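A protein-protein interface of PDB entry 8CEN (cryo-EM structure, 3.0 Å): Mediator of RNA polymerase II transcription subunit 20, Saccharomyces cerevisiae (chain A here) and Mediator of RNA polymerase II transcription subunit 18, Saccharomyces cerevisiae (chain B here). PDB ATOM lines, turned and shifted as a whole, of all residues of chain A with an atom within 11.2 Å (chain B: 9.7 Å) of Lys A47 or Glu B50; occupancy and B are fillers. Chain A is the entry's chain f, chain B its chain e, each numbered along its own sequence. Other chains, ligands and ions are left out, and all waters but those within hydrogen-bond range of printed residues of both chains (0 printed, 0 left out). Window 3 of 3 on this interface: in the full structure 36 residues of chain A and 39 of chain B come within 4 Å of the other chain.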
ATOM      1  N   ARG A  43     -23.649  17.959   4.248  1.00  0.00           N
ATOM      2  CA  ARG A  43     -23.470  18.630   5.525  1.00  0.00           C
ATOM      3  C   ARG A  43     -22.098  18.285   6.086  1.00  0.00           C
ATOM      4  O   ARG A  43     -21.659  17.133   6.017  1.00  0.00           O
ATOM      5  CB  ARG A  43     -24.557  18.217   6.518  1.00  0.00           C
ATOM      6  CG  ARG A  43     -25.870  18.981   6.402  1.00  0.00           C
ATOM      7  CD  ARG A  43     -25.880  20.246   7.242  1.00  0.00           C
ATOM      8  NE  ARG A  43     -26.851  21.219   6.754  1.00  0.00           N
ATOM      9  CZ  ARG A  43     -26.936  22.471   7.181  1.00  0.00           C
ATOM     10  NH1 ARG A  43     -26.097  22.951   8.084  1.00  0.00           N
ATOM     11  NH2 ARG A  43     -27.895  23.256   6.700  1.00  0.00           N
ATOM     12  N   CYS A  44     -21.416  19.295   6.619  1.00  0.00           N
ATOM     13  CA  CYS A  44     -20.107  19.090   7.220  1.00  0.00           C
ATOM     14  C   CYS A  44     -20.268  18.490   8.611  1.00  0.00           C
ATOM     15  O   CYS A  44     -21.067  18.976   9.418  1.00  0.00           O
ATOM     16  CB  CYS A  44     -19.342  20.411   7.290  1.00  0.00           C
ATOM     17  SG  CYS A  44     -17.615  20.246   7.778  1.00  0.00           S
ATOM     18  N   SER A  45     -19.505  17.432   8.890  1.00  0.00           N
ATOM     19  CA  SER A  45     -19.617  16.685  10.134  1.00  0.00           C
ATOM     20  C   SER A  45     -18.500  17.012  11.120  1.00  0.00           C
ATOM     21  O   SER A  45     -18.262  16.239  12.054  1.00  0.00           O
ATOM     22  CB  SER A  45     -19.642  15.184   9.846  1.00  0.00           C
ATOM     23  OG  SER A  45     -18.395  14.739   9.344  1.00  0.00           O
ATOM     24  N   ILE A  46     -17.810  18.138  10.932  1.00  0.00           N
ATOM     25  CA  ILE A  46     -16.772  18.545  11.872  1.00  0.00           C
ATOM     26  C   ILE A  46     -17.426  19.045  13.153  1.00  0.00           C
ATOM     27  O   ILE A  46     -18.330  19.893  13.119  1.00  0.00           O
ATOM     28  CB  ILE A  46     -15.866  19.614  11.244  1.00  0.00           C
ATOM     29  CG1 ILE A  46     -15.085  19.026  10.066  1.00  0.00           C
ATOM     30  CG2 ILE A  46     -14.904  20.188  12.277  1.00  0.00           C
ATOM     31  CD1 ILE A  46     -14.277  17.799  10.416  1.00  0.00           C
ATOM     32  N   LYS A  47     -16.979  18.510  14.293  1.00  0.00           N
ATOM     33  CA  LYS A  47     -17.590  18.854  15.573  1.00  0.00           C
ATOM     34  C   LYS A  47     -17.299  20.292  15.984  1.00  0.00           C
ATOM     35  O   LYS A  47     -18.158  20.946  16.587  1.00  0.00           O
ATOM     36  CB  LYS A  47     -17.107  17.892  16.661  1.00  0.00           C
ATOM     37  CG  LYS A  47     -17.540  16.446  16.466  1.00  0.00           C
ATOM     38  CD  LYS A  47     -19.038  16.332  16.237  1.00  0.00           C
ATOM     39  CE  LYS A  47     -19.453  14.883  16.032  1.00  0.00           C
ATOM     40  NZ  LYS A  47     -20.908  14.755  15.741  1.00  0.00           N
ATOM     41  N   ASN A  48     -16.109  20.802  15.675  1.00  0.00           N
ATOM     42  CA  ASN A  48     -15.675  22.126  16.122  1.00  0.00           C
ATOM     43  C   ASN A  48     -15.351  22.994  14.907  1.00  0.00           C
ATOM     44  O   ASN A  48     -14.206  23.058  14.453  1.00  0.00           O
ATOM     45  CB  ASN A  48     -14.475  22.005  17.074  1.00  0.00           C
ATOM     46  CG  ASN A  48     -13.430  21.021  16.579  1.00  0.00           C
ATOM     47  OD1 ASN A  48     -13.557  20.460  15.491  1.00  0.00           O
ATOM     48  ND2 ASN A  48     -12.392  20.806  17.379  1.00  0.00           N
ATOM     49  N   LEU A  49     -16.365  23.673  14.385  1.00  0.00           N
ATOM     50  CA  LEU A  49     -16.118  24.616  13.311  1.00  0.00           C
ATOM     51  C   LEU A  49     -16.208  26.047  13.832  1.00  0.00           C
ATOM     52  O   LEU A  49     -17.039  26.348  14.695  1.00  0.00           O
ATOM     53  CB  LEU A  49     -17.113  24.429  12.159  1.00  0.00           C
ATOM     54  CG  LEU A  49     -16.747  23.348  11.140  1.00  0.00           C
ATOM     55  CD1 LEU A  49     -17.793  23.262  10.042  1.00  0.00           C
ATOM     56  CD2 LEU A  49     -15.371  23.606  10.550  1.00  0.00           C
ATOM     57  N   PRO A  50     -15.366  26.957  13.329  1.00  0.00           N
ATOM     58  CA  PRO A  50     -15.411  28.346  13.806  1.00  0.00           C
ATOM     59  C   PRO A  50     -16.591  29.127  13.250  1.00  0.00           C
ATOM     60  O   PRO A  50     -17.472  28.561  12.596  1.00  0.00           O
ATOM     61  CB  PRO A  50     -14.076  28.923  13.320  1.00  0.00           C
ATOM     62  CG  PRO A  50     -13.754  28.125  12.106  1.00  0.00           C
ATOM     63  CD  PRO A  50     -14.264  26.735  12.374  1.00  0.00           C
ATOM     64  N   ALA A  51     -16.626  30.429  13.518  1.00  0.00           N
ATOM     65  CA  ALA A  51     -17.692  31.270  13.006  1.00  0.00           C
ATOM     66  C   ALA A  51     -17.419  31.664  11.555  1.00  0.00           C
ATOM     67  O   ALA A  51     -16.306  31.511  11.040  1.00  0.00           O
ATOM     68  CB  ALA A  51     -17.856  32.515  13.877  1.00  0.00           C
ATOM     69  N   VAL A  53     -18.416  30.398   8.736  1.00  0.00           N
ATOM     70  CA  VAL A  53     -18.212  29.323   7.770  1.00  0.00           C
ATOM     71  C   VAL A  53     -19.487  28.485   7.725  1.00  0.00           C
ATOM     72  O   VAL A  53     -20.151  28.284   8.749  1.00  0.00           O
ATOM     73  CB  VAL A  53     -16.958  28.474   8.106  1.00  0.00           C
ATOM     74  CG1 VAL A  53     -17.081  27.779   9.455  1.00  0.00           C
ATOM     75  CG2 VAL A  53     -16.647  27.474   6.992  1.00  0.00           C
ATOM     76  N   LYS A  55     -21.736  24.991   6.704  1.00  0.00           N
ATOM     77  CA  LYS A  55     -21.655  23.539   6.628  1.00  0.00           C
ATOM     78  C   LYS A  55     -22.388  22.968   5.423  1.00  0.00           C
ATOM     79  O   LYS A  55     -22.471  21.745   5.289  1.00  0.00           O
ATOM     80  CB  LYS A  55     -22.213  22.909   7.909  1.00  0.00           C
ATOM     81  CG  LYS A  55     -21.404  23.203   9.157  1.00  0.00           C
ATOM     82  CD  LYS A  55     -22.012  22.534  10.377  1.00  0.00           C
ATOM     83  CE  LYS A  55     -21.152  22.752  11.611  1.00  0.00           C
ATOM     84  NZ  LYS A  55     -21.128  24.182  12.022  1.00  0.00           N
ATOM     85  N   SER A 110     -17.818   7.976  -0.628  1.00  0.00           N
ATOM     86  CA  SER A 110     -17.046   6.789  -0.289  1.00  0.00           C
ATOM     87  C   SER A 110     -15.890   7.096   0.653  1.00  0.00           C
ATOM     88  O   SER A 110     -15.807   6.508   1.735  1.00  0.00           O
ATOM     89  CB  SER A 110     -16.522   6.121  -1.569  1.00  0.00           C
ATOM     90  OG  SER A 110     -15.535   6.923  -2.193  1.00  0.00           O
ATOM     91  N   LYS A 111     -14.990   8.007   0.276  1.00  0.00           N
ATOM     92  CA  LYS A 111     -13.743   8.201   1.005  1.00  0.00           C
ATOM     93  C   LYS A 111     -13.539   9.608   1.550  1.00  0.00           C
ATOM     94  O   LYS A 111     -12.509   9.861   2.185  1.00  0.00           O
ATOM     95  CB  LYS A 111     -12.557   7.802   0.118  1.00  0.00           C
ATOM     96  CG  LYS A 111     -12.368   8.665  -1.101  1.00  0.00           C
ATOM     97  CD  LYS A 111     -11.164   8.218  -1.885  1.00  0.00           C
ATOM     98  CE  LYS A 111     -11.445   6.902  -2.578  1.00  0.00           C
ATOM     99  NZ  LYS A 111     -12.494   7.042  -3.619  1.00  0.00           N
ATOM    100  N   LEU A 112     -14.471  10.530   1.312  1.00  0.00           N
ATOM    101  CA  LEU A 112     -14.476  11.822   1.988  1.00  0.00           C
ATOM    102  C   LEU A 112     -15.693  11.975   2.892  1.00  0.00           C
ATOM    103  O   LEU A 112     -16.093  13.100   3.206  1.00  0.00           O
ATOM    104  CB  LEU A 112     -14.422  12.972   0.978  1.00  0.00           C
ATOM    105  CG  LEU A 112     -13.219  13.054   0.038  1.00  0.00           C
ATOM    106  CD1 LEU A 112     -13.335  14.264  -0.869  1.00  0.00           C
ATOM    107  CD2 LEU A 112     -11.925  13.108   0.834  1.00  0.00           C
ATOM    108  N   SER A 113     -16.283  10.861   3.322  1.00  0.00           N
ATOM    109  CA  SER A 113     -17.508  10.893   4.107  1.00  0.00           C
ATOM    110  C   SER A 113     -17.278  11.233   5.572  1.00  0.00           C
ATOM    111  O   SER A 113     -18.249  11.517   6.280  1.00  0.00           O
ATOM    112  CB  SER A 113     -18.234   9.554   4.004  1.00  0.00           C
ATOM    113  OG  SER A 113     -18.555   9.257   2.660  1.00  0.00           O
ATOM    114  N   ASN A 114     -16.030  11.206   6.047  1.00  0.00           N
ATOM    115  CA  ASN A 114     -15.754  11.664   7.402  1.00  0.00           C
ATOM    116  C   ASN A 114     -15.876  13.176   7.529  1.00  0.00           C
ATOM    117  O   ASN A 114     -16.034  13.683   8.644  1.00  0.00           O
ATOM    118  CB  ASN A 114     -14.361  11.211   7.845  1.00  0.00           C
ATOM    119  CG  ASN A 114     -13.297  11.484   6.801  1.00  0.00           C
ATOM    120  OD1 ASN A 114     -13.597  11.927   5.693  1.00  0.00           O
ATOM    121  ND2 ASN A 114     -12.043  11.220   7.151  1.00  0.00           N
ATOM    122  N   ILE A 115     -15.811  13.901   6.417  1.00  0.00           N
ATOM    123  CA  ILE A 115     -15.945  15.352   6.409  1.00  0.00           C
ATOM    124  C   ILE A 115     -17.325  15.784   5.927  1.00  0.00           C
ATOM    125  O   ILE A 115     -17.995  16.583   6.581  1.00  0.00           O
ATOM    126  CB  ILE A 115     -14.830  15.985   5.547  1.00  0.00           C
ATOM    127  CG1 ILE A 115     -13.472  15.366   5.887  1.00  0.00           C
ATOM    128  CG2 ILE A 115     -14.803  17.494   5.734  1.00  0.00           C
ATOM    129  CD1 ILE A 115     -12.981  15.693   7.279  1.00  0.00           C
ATOM    130  N   TRP A 116     -17.767  15.263   4.785  1.00  0.00           N
ATOM    131  CA  TRP A 116     -19.030  15.654   4.173  1.00  0.00           C
ATOM    132  C   TRP A 116     -19.962  14.453   4.107  1.00  0.00           C
ATOM    133  O   TRP A 116     -19.575  13.393   3.608  1.00  0.00           O
ATOM    134  CB  TRP A 116     -18.806  16.217   2.767  1.00  0.00           C
ATOM    135  CG  TRP A 116     -18.043  17.499   2.753  1.00  0.00           C
ATOM    136  CD1 TRP A 116     -16.724  17.665   2.450  1.00  0.00           C
ATOM    137  CD2 TRP A 116     -18.551  18.801   3.060  1.00  0.00           C
ATOM    138  NE1 TRP A 116     -16.379  18.990   2.547  1.00  0.00           N
ATOM    139  CE2 TRP A 116     -17.484  19.709   2.920  1.00  0.00           C
ATOM    140  CE3 TRP A 116     -19.806  19.287   3.439  1.00  0.00           C
ATOM    141  CZ2 TRP A 116     -17.634  21.073   3.147  1.00  0.00           C
ATOM    142  CZ3 TRP A 116     -19.952  20.640   3.662  1.00  0.00           C
ATOM    143  CH2 TRP A 116     -18.873  21.519   3.516  1.00  0.00           C
ATOM    144  N   MET A 117     -21.189  14.624   4.590  1.00  0.00           N
ATOM    145  CA  MET A 117     -22.195  13.571   4.553  1.00  0.00           C
ATOM    146  C   MET A 117     -23.358  14.009   3.675  1.00  0.00           C
ATOM    147  O   MET A 117     -23.902  15.102   3.861  1.00  0.00           O
ATOM    148  CB  MET A 117     -22.693  13.230   5.960  1.00  0.00           C
ATOM    149  CG  MET A 117     -23.707  12.099   5.998  1.00  0.00           C
ATOM    150  SD  MET A 117     -24.254  11.708   7.670  1.00  0.00           S
ATOM    151  CE  MET A 117     -25.270  13.137   8.034  1.00  0.00           C
ATOM    152  N   PRO B  43      -5.807  16.484   5.847  1.00  0.00           N
ATOM    153  CA  PRO B  43      -6.962  17.034   6.570  1.00  0.00           C
ATOM    154  C   PRO B  43      -6.539  17.974   7.690  1.00  0.00           C
ATOM    155  O   PRO B  43      -5.462  17.835   8.275  1.00  0.00           O
ATOM    156  CB  PRO B  43      -7.669  15.788   7.118  1.00  0.00           C
ATOM    157  CG  PRO B  43      -6.643  14.716   7.087  1.00  0.00           C
ATOM    158  CD  PRO B  43      -5.793  15.011   5.898  1.00  0.00           C
ATOM    159  N   ASN B  44      -7.398  18.953   7.958  1.00  0.00           N
ATOM    160  CA  ASN B  44      -7.077  20.062   8.849  1.00  0.00           C
ATOM    161  C   ASN B  44      -6.875  19.568  10.278  1.00  0.00           C
ATOM    162  O   ASN B  44      -7.783  18.938  10.841  1.00  0.00           O
ATOM    163  CB  ASN B  44      -8.197  21.099   8.799  1.00  0.00           C
ATOM    164  CG  ASN B  44      -7.725  22.496   9.158  1.00  0.00           C
ATOM    165  OD1 ASN B  44      -6.916  22.680  10.067  1.00  0.00           O
ATOM    166  ND2 ASN B  44      -8.235  23.491   8.443  1.00  0.00           N
ATOM    167  N   SER B  46      -6.893  21.297  12.940  1.00  0.00           N
ATOM    168  CA  SER B  46      -7.810  22.016  13.814  1.00  0.00           C
ATOM    169  C   SER B  46      -9.239  21.499  13.723  1.00  0.00           C
ATOM    170  O   SER B  46     -10.091  21.942  14.500  1.00  0.00           O
ATOM    171  CB  SER B  46      -7.783  23.511  13.486  1.00  0.00           C
ATOM    172  OG  SER B  46      -8.154  23.744  12.139  1.00  0.00           O
ATOM    173  N   TYR B  47      -9.520  20.584  12.799  1.00  0.00           N
ATOM    174  CA  TYR B  47     -10.851  20.020  12.623  1.00  0.00           C
ATOM    175  C   TYR B  47     -10.907  18.673  13.330  1.00  0.00           C
ATOM    176  O   TYR B  47     -10.111  17.777  13.026  1.00  0.00           O
ATOM    177  CB  TYR B  47     -11.187  19.851  11.140  1.00  0.00           C
ATOM    178  CG  TYR B  47     -11.493  21.130  10.383  1.00  0.00           C
ATOM    179  CD1 TYR B  47     -11.475  22.369  11.015  1.00  0.00           C
ATOM    180  CD2 TYR B  47     -11.803  21.093   9.028  1.00  0.00           C
ATOM    181  CE1 TYR B  47     -11.752  23.531  10.318  1.00  0.00           C
ATOM    182  CE2 TYR B  47     -12.084  22.249   8.324  1.00  0.00           C
ATOM    183  CZ  TYR B  47     -12.057  23.465   8.975  1.00  0.00           C
ATOM    184  OH  TYR B  47     -12.337  24.618   8.276  1.00  0.00           O
ATOM    185  N   ASP B  48     -11.840  18.528  14.267  1.00  0.00           N
ATOM    186  CA  ASP B  48     -12.043  17.245  14.928  1.00  0.00           C
ATOM    187  C   ASP B  48     -12.835  16.339  13.995  1.00  0.00           C
ATOM    188  O   ASP B  48     -13.963  16.665  13.609  1.00  0.00           O
ATOM    189  CB  ASP B  48     -12.771  17.425  16.259  1.00  0.00           C
ATOM    190  CG  ASP B  48     -12.547  16.264  17.212  1.00  0.00           C
ATOM    191  OD1 ASP B  48     -12.073  15.199  16.764  1.00  0.00           O
ATOM    192  OD2 ASP B  48     -12.847  16.418  18.415  1.00  0.00           O
ATOM    193  N   VAL B  49     -12.244  15.206  13.633  1.00  0.00           N
ATOM    194  CA  VAL B  49     -12.848  14.281  12.691  1.00  0.00           C
ATOM    195  C   VAL B  49     -13.257  13.015  13.437  1.00  0.00           C
ATOM    196  O   VAL B  49     -12.844  12.767  14.569  1.00  0.00           O
ATOM    197  CB  VAL B  49     -11.904  13.951  11.519  1.00  0.00           C
ATOM    198  CG1 VAL B  49     -11.573  15.209  10.736  1.00  0.00           C
ATOM    199  CG2 VAL B  49     -10.637  13.285  12.031  1.00  0.00           C
ATOM    200  N   GLU B  50     -14.089  12.212  12.784  1.00  0.00           N
ATOM    201  CA  GLU B  50     -14.501  10.916  13.298  1.00  0.00           C
ATOM    202  C   GLU B  50     -13.838   9.823  12.474  1.00  0.00           C
ATOM    203  O   GLU B  50     -13.678   9.961  11.257  1.00  0.00           O
ATOM    204  CB  GLU B  50     -16.024  10.762  13.252  1.00  0.00           C
ATOM    205  CG  GLU B  50     -16.778  11.741  14.141  1.00  0.00           C
ATOM    206  CD  GLU B  50     -16.535  11.502  15.618  1.00  0.00           C
ATOM    207  OE1 GLU B  50     -16.373  10.329  16.014  1.00  0.00           O
ATOM    208  OE2 GLU B  50     -16.502  12.489  16.383  1.00  0.00           O
ATOM    209  N   ASN B  51     -13.438   8.741  13.147  1.00  0.00           N
ATOM    210  CA  ASN B  51     -12.815   7.622  12.449  1.00  0.00           C
ATOM    211  C   ASN B  51     -13.800   6.919  11.526  1.00  0.00           C
ATOM    212  O   ASN B  51     -13.393   6.331  10.518  1.00  0.00           O
ATOM    213  CB  ASN B  51     -12.234   6.631  13.458  1.00  0.00           C
ATOM    214  CG  ASN B  51     -11.315   7.295  14.462  1.00  0.00           C
ATOM    215  OD1 ASN B  51     -11.580   7.286  15.664  1.00  0.00           O
ATOM    216  ND2 ASN B  51     -10.227   7.879  13.973  1.00  0.00           N
ATOM    217  N   VAL B  52     -15.090   6.975  11.847  1.00  0.00           N
ATOM    218  CA  VAL B  52     -16.126   6.389  11.008  1.00  0.00           C
ATOM    219  C   VAL B  52     -16.457   7.348   9.872  1.00  0.00           C
ATOM    220  O   VAL B  52     -16.064   8.520   9.892  1.00  0.00           O
ATOM    221  CB  VAL B  52     -17.382   6.046  11.830  1.00  0.00           C
ATOM    222  CG1 VAL B  52     -17.010   5.187  13.028  1.00  0.00           C
ATOM    223  CG2 VAL B  52     -18.089   7.316  12.279  1.00  0.00           C
ATOM    224  N   ASN B  53     -17.186   6.850   8.878  1.00  0.00           N
ATOM    225  CA  ASN B  53     -17.637   7.646   7.743  1.00  0.00           C
ATOM    226  C   ASN B  53     -19.162   7.693   7.749  1.00  0.00           C
ATOM    227  O   ASN B  53     -19.772   7.477   8.801  1.00  0.00           O
ATOM    228  CB  ASN B  53     -17.046   7.116   6.425  1.00  0.00           C
ATOM    229  CG  ASN B  53     -17.315   5.636   6.183  1.00  0.00           C
ATOM    230  OD1 ASN B  53     -18.419   5.139   6.371  1.00  0.00           O
ATOM    231  ND2 ASN B  53     -16.280   4.926   5.748  1.00  0.00           N
ATOM    232  N   SER B  54     -19.774   8.097   6.631  1.00  0.00           N
ATOM    233  CA  SER B  54     -21.235   8.120   6.539  1.00  0.00           C
ATOM    234  C   SER B  54     -21.848   6.747   6.805  1.00  0.00           C
ATOM    235  O   SER B  54     -22.926   6.654   7.404  1.00  0.00           O
ATOM    236  CB  SER B  54     -21.665   8.630   5.165  1.00  0.00           C
ATOM    237  OG  SER B  54     -21.167   7.794   4.134  1.00  0.00           O
ATOM    238  N   ARG B  55     -21.184   5.680   6.373  1.00  0.00           N
ATOM    239  CA  ARG B  55     -21.578   4.317   6.691  1.00  0.00           C
ATOM    240  C   ARG B  55     -20.824   3.915   7.970  1.00  0.00           C
ATOM    241  O   ARG B  55     -20.153   4.741   8.589  1.00  0.00           O
ATOM    242  CB  ARG B  55     -21.348   3.460   5.439  1.00  0.00           C
ATOM    243  CG  ARG B  55     -21.854   2.025   5.441  1.00  0.00           C
ATOM    244  CD  ARG B  55     -20.666   1.095   5.384  1.00  0.00           C
ATOM    245  NE  ARG B  55     -21.033  -0.306   5.238  1.00  0.00           N
ATOM    246  CZ  ARG B  55     -21.156  -1.145   6.257  1.00  0.00           C
ATOM    247  NH1 ARG B  55     -20.924  -0.754   7.500  1.00  0.00           N
ATOM    248  NH2 ARG B  55     -21.503  -2.407   6.023  1.00  0.00           N
ATOM    249  N   GLN B  57     -18.307   1.883   8.478  1.00  0.00           N
ATOM    250  CA  GLN B  57     -16.933   1.430   8.297  1.00  0.00           C
ATOM    251  C   GLN B  57     -15.950   2.515   8.719  1.00  0.00           C
ATOM    252  O   GLN B  57     -16.068   3.669   8.295  1.00  0.00           O
ATOM    253  CB  GLN B  57     -16.702   1.028   6.842  1.00  0.00           C
ATOM    254  CG  GLN B  57     -17.490  -0.202   6.430  1.00  0.00           C
ATOM    255  CD  GLN B  57     -17.283  -0.580   4.979  1.00  0.00           C
ATOM    256  OE1 GLN B  57     -16.596   0.117   4.235  1.00  0.00           O
ATOM    257  NE2 GLN B  57     -17.883  -1.689   4.566  1.00  0.00           N
ATOM    258  N   LEU B  58     -14.984   2.138   9.553  1.00  0.00           N
ATOM    259  CA  LEU B  58     -13.994   3.068  10.084  1.00  0.00           C
ATOM    260  C   LEU B  58     -12.795   3.170   9.147  1.00  0.00           C
ATOM    261  O   LEU B  58     -12.272   2.154   8.678  1.00  0.00           O
ATOM    262  CB  LEU B  58     -13.588   2.640  11.501  1.00  0.00           C
ATOM    263  CG  LEU B  58     -12.938   1.294  11.862  1.00  0.00           C
ATOM    264  CD1 LEU B  58     -11.433   1.248  11.672  1.00  0.00           C
ATOM    265  CD2 LEU B  58     -13.297   0.915  13.293  1.00  0.00           C
ATOM    266  N   VAL B  59     -12.388   4.407   8.847  1.00  0.00           N
ATOM    267  CA  VAL B  59     -11.313   4.692   7.902  1.00  0.00           C
ATOM    268  C   VAL B  59     -10.318   5.655   8.538  1.00  0.00           C
ATOM    269  O   VAL B  59     -10.636   6.368   9.495  1.00  0.00           O
ATOM    270  CB  VAL B  59     -11.840   5.275   6.566  1.00  0.00           C
ATOM    271  CG1 VAL B  59     -12.856   4.343   5.917  1.00  0.00           C
ATOM    272  CG2 VAL B  59     -12.449   6.652   6.787  1.00  0.00           C
ATOM    273  N   GLU B  60      -9.040   5.656   7.983  1.00  0.00           N
ATOM    274  CA  GLU B  60      -7.969   6.584   8.318  1.00  0.00           C
ATOM    275  C   GLU B  60      -8.070   7.859   7.486  1.00  0.00           C
ATOM    276  O   GLU B  60      -8.556   7.830   6.350  1.00  0.00           O
ATOM    277  CB  GLU B  60      -6.601   5.946   8.075  1.00  0.00           C
ATOM    278  CG  GLU B  60      -6.015   5.205   9.262  1.00  0.00           C
ATOM    279  CD  GLU B  60      -6.021   6.034  10.532  1.00  0.00           C
ATOM    280  OE1 GLU B  60      -5.286   7.042  10.591  1.00  0.00           O
ATOM    281  OE2 GLU B  60      -6.762   5.678  11.473  1.00  0.00           O
ATOM    282  N   PRO B  61      -7.631   8.989   8.039  1.00  0.00           N
ATOM    283  CA  PRO B  61      -7.423  10.179   7.205  1.00  0.00           C
ATOM    284  C   PRO B  61      -6.307   9.943   6.198  1.00  0.00           C
ATOM    285  O   PRO B  61      -5.322   9.257   6.484  1.00  0.00           O
ATOM    286  CB  PRO B  61      -7.048  11.265   8.219  1.00  0.00           C
ATOM    287  CG  PRO B  61      -7.562  10.768   9.528  1.00  0.00           C
ATOM    288  CD  PRO B  61      -7.451   9.277   9.470  1.00  0.00           C
ATOM    289  N   ASN B  62      -6.467  10.521   5.011  1.00  0.00           N
ATOM    290  CA  ASN B  62      -5.550  10.296   3.904  1.00  0.00           C
ATOM    291  C   ASN B  62      -5.174  11.622   3.262  1.00  0.00           C
ATOM    292  O   ASN B  62      -6.026  12.496   3.083  1.00  0.00           O
ATOM    293  CB  ASN B  62      -6.177   9.367   2.855  1.00  0.00           C
ATOM    294  CG  ASN B  62      -5.147   8.729   1.945  1.00  0.00           C
ATOM    295  OD1 ASN B  62      -3.953   9.012   2.043  1.00  0.00           O
ATOM    296  ND2 ASN B  62      -5.605   7.864   1.048  1.00  0.00           N
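Ile A46 touches Tyr B47 (CD1 to CB, 3.8 Å).
Asp B48 touches Ile A46.
Ile A46 touches Val B49.
N of Lys A47 touches O of Asp B48, at 3.6 Å.
Lys A47 touches Glu B50.
Ser B46 touches Asn A48 (O to ND2, 3.9 Å).
Asn A48 touches Tyr B47.
Asn A114 touches Glu B50.
Asn A114 touches Val B52.
CG1 of Val B49 touches CD1 of Ile A115, at 3.8 Å.
N of Asp B48 is in hydrogen-bond range of OD1 of Asn A48, at 2.9 Å.
The side-chain hydroxyl (OG) of Ser B54 sits at hydrogen-bond distance from the side-chain hydroxyl (OG) of Ser A113, 3.3 Å away.
Of chain B, only Tyr B47 (3.8 Å), Asp B48 (3.4 Å) and Val B49 (3.8 Å) come within 4 Å of Ile A46.
Of chain B, only Asp B48 and Glu B50 come within 4 Å of Lys A47.
Printed residues of chain B within 4 Å of Asn A48: Ser B46, Tyr B47 and Asp B48.
Of the printed residues of chain B, Leu A49 touches Tyr B47.
Pro A50 touches none of the printed residues of chain B.
Printed residues of chain A within 4 Å of Ser B46: Asn A48.
Printed residues of chain A within 4 Å of Tyr B47: Ile A46, Asn A48 and Leu A49.
Printed residues of chain A within 4 Å of Asp B48: Ile A46, Lys A47 and Asn A48.
Val B49 touches two residues of chain A.
Of chain A, only Lys A47 (3.8 Å) and Asn A114 (3.7 Å) come within 4 Å of Glu B50.
No residue of chain A comes within 4 Å of Asn B51.
Val B52 touches just one residue of chain A: Asn A114 (3.8 Å).
Of the printed residues of chain A, Asn B53 touches Ser A113.
The nearest residue of chain B that does not touch Lys A47 is Val B49 (5.8 Å).
Hydrophobic or aromatic side chains of chain A that line the printed part of chain B: Ile A46, Leu A49 and Ile A115.
Along chain A the printed residues that touch a printed residue of chain B span positions 46 to 115.
Of the 18 printed residues of chain B, 8 touch a printed residue of chain A.
Hydrophobic or aromatic side chains of chain B that line the printed part of chain A: Tyr B47 and Val B49.
Along chain B the printed residues that touch a printed residue of chain A span positions 46 to 54.
Among the printed residues, no Asp or Glu carboxylate lies within 4 Å of a Lys or Arg side-chain nitrogen of the other chain.
The side-chain hydroxyl (OG) of Ser B46 lies within hydrogen-bond range of the side-chain amide oxygen (OD1) of Asn B44 (2.6 Å).
OD1 of Asn B53 lies within hydrogen-bond range of N of Arg B55.
ND2 of Asn B53 sits at hydrogen-bond distance from O of Gln B57.
N of Ile A46 sits close to SG of Cys A44.
OG of Ser A45 sits at hydrogen-bond distance from O of Asn A114.
The backbone carbonyl oxygen (O) of Ile A115 lies within hydrogen-bond range of the backbone NH (N) of Ser A45 (2.9 Å).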
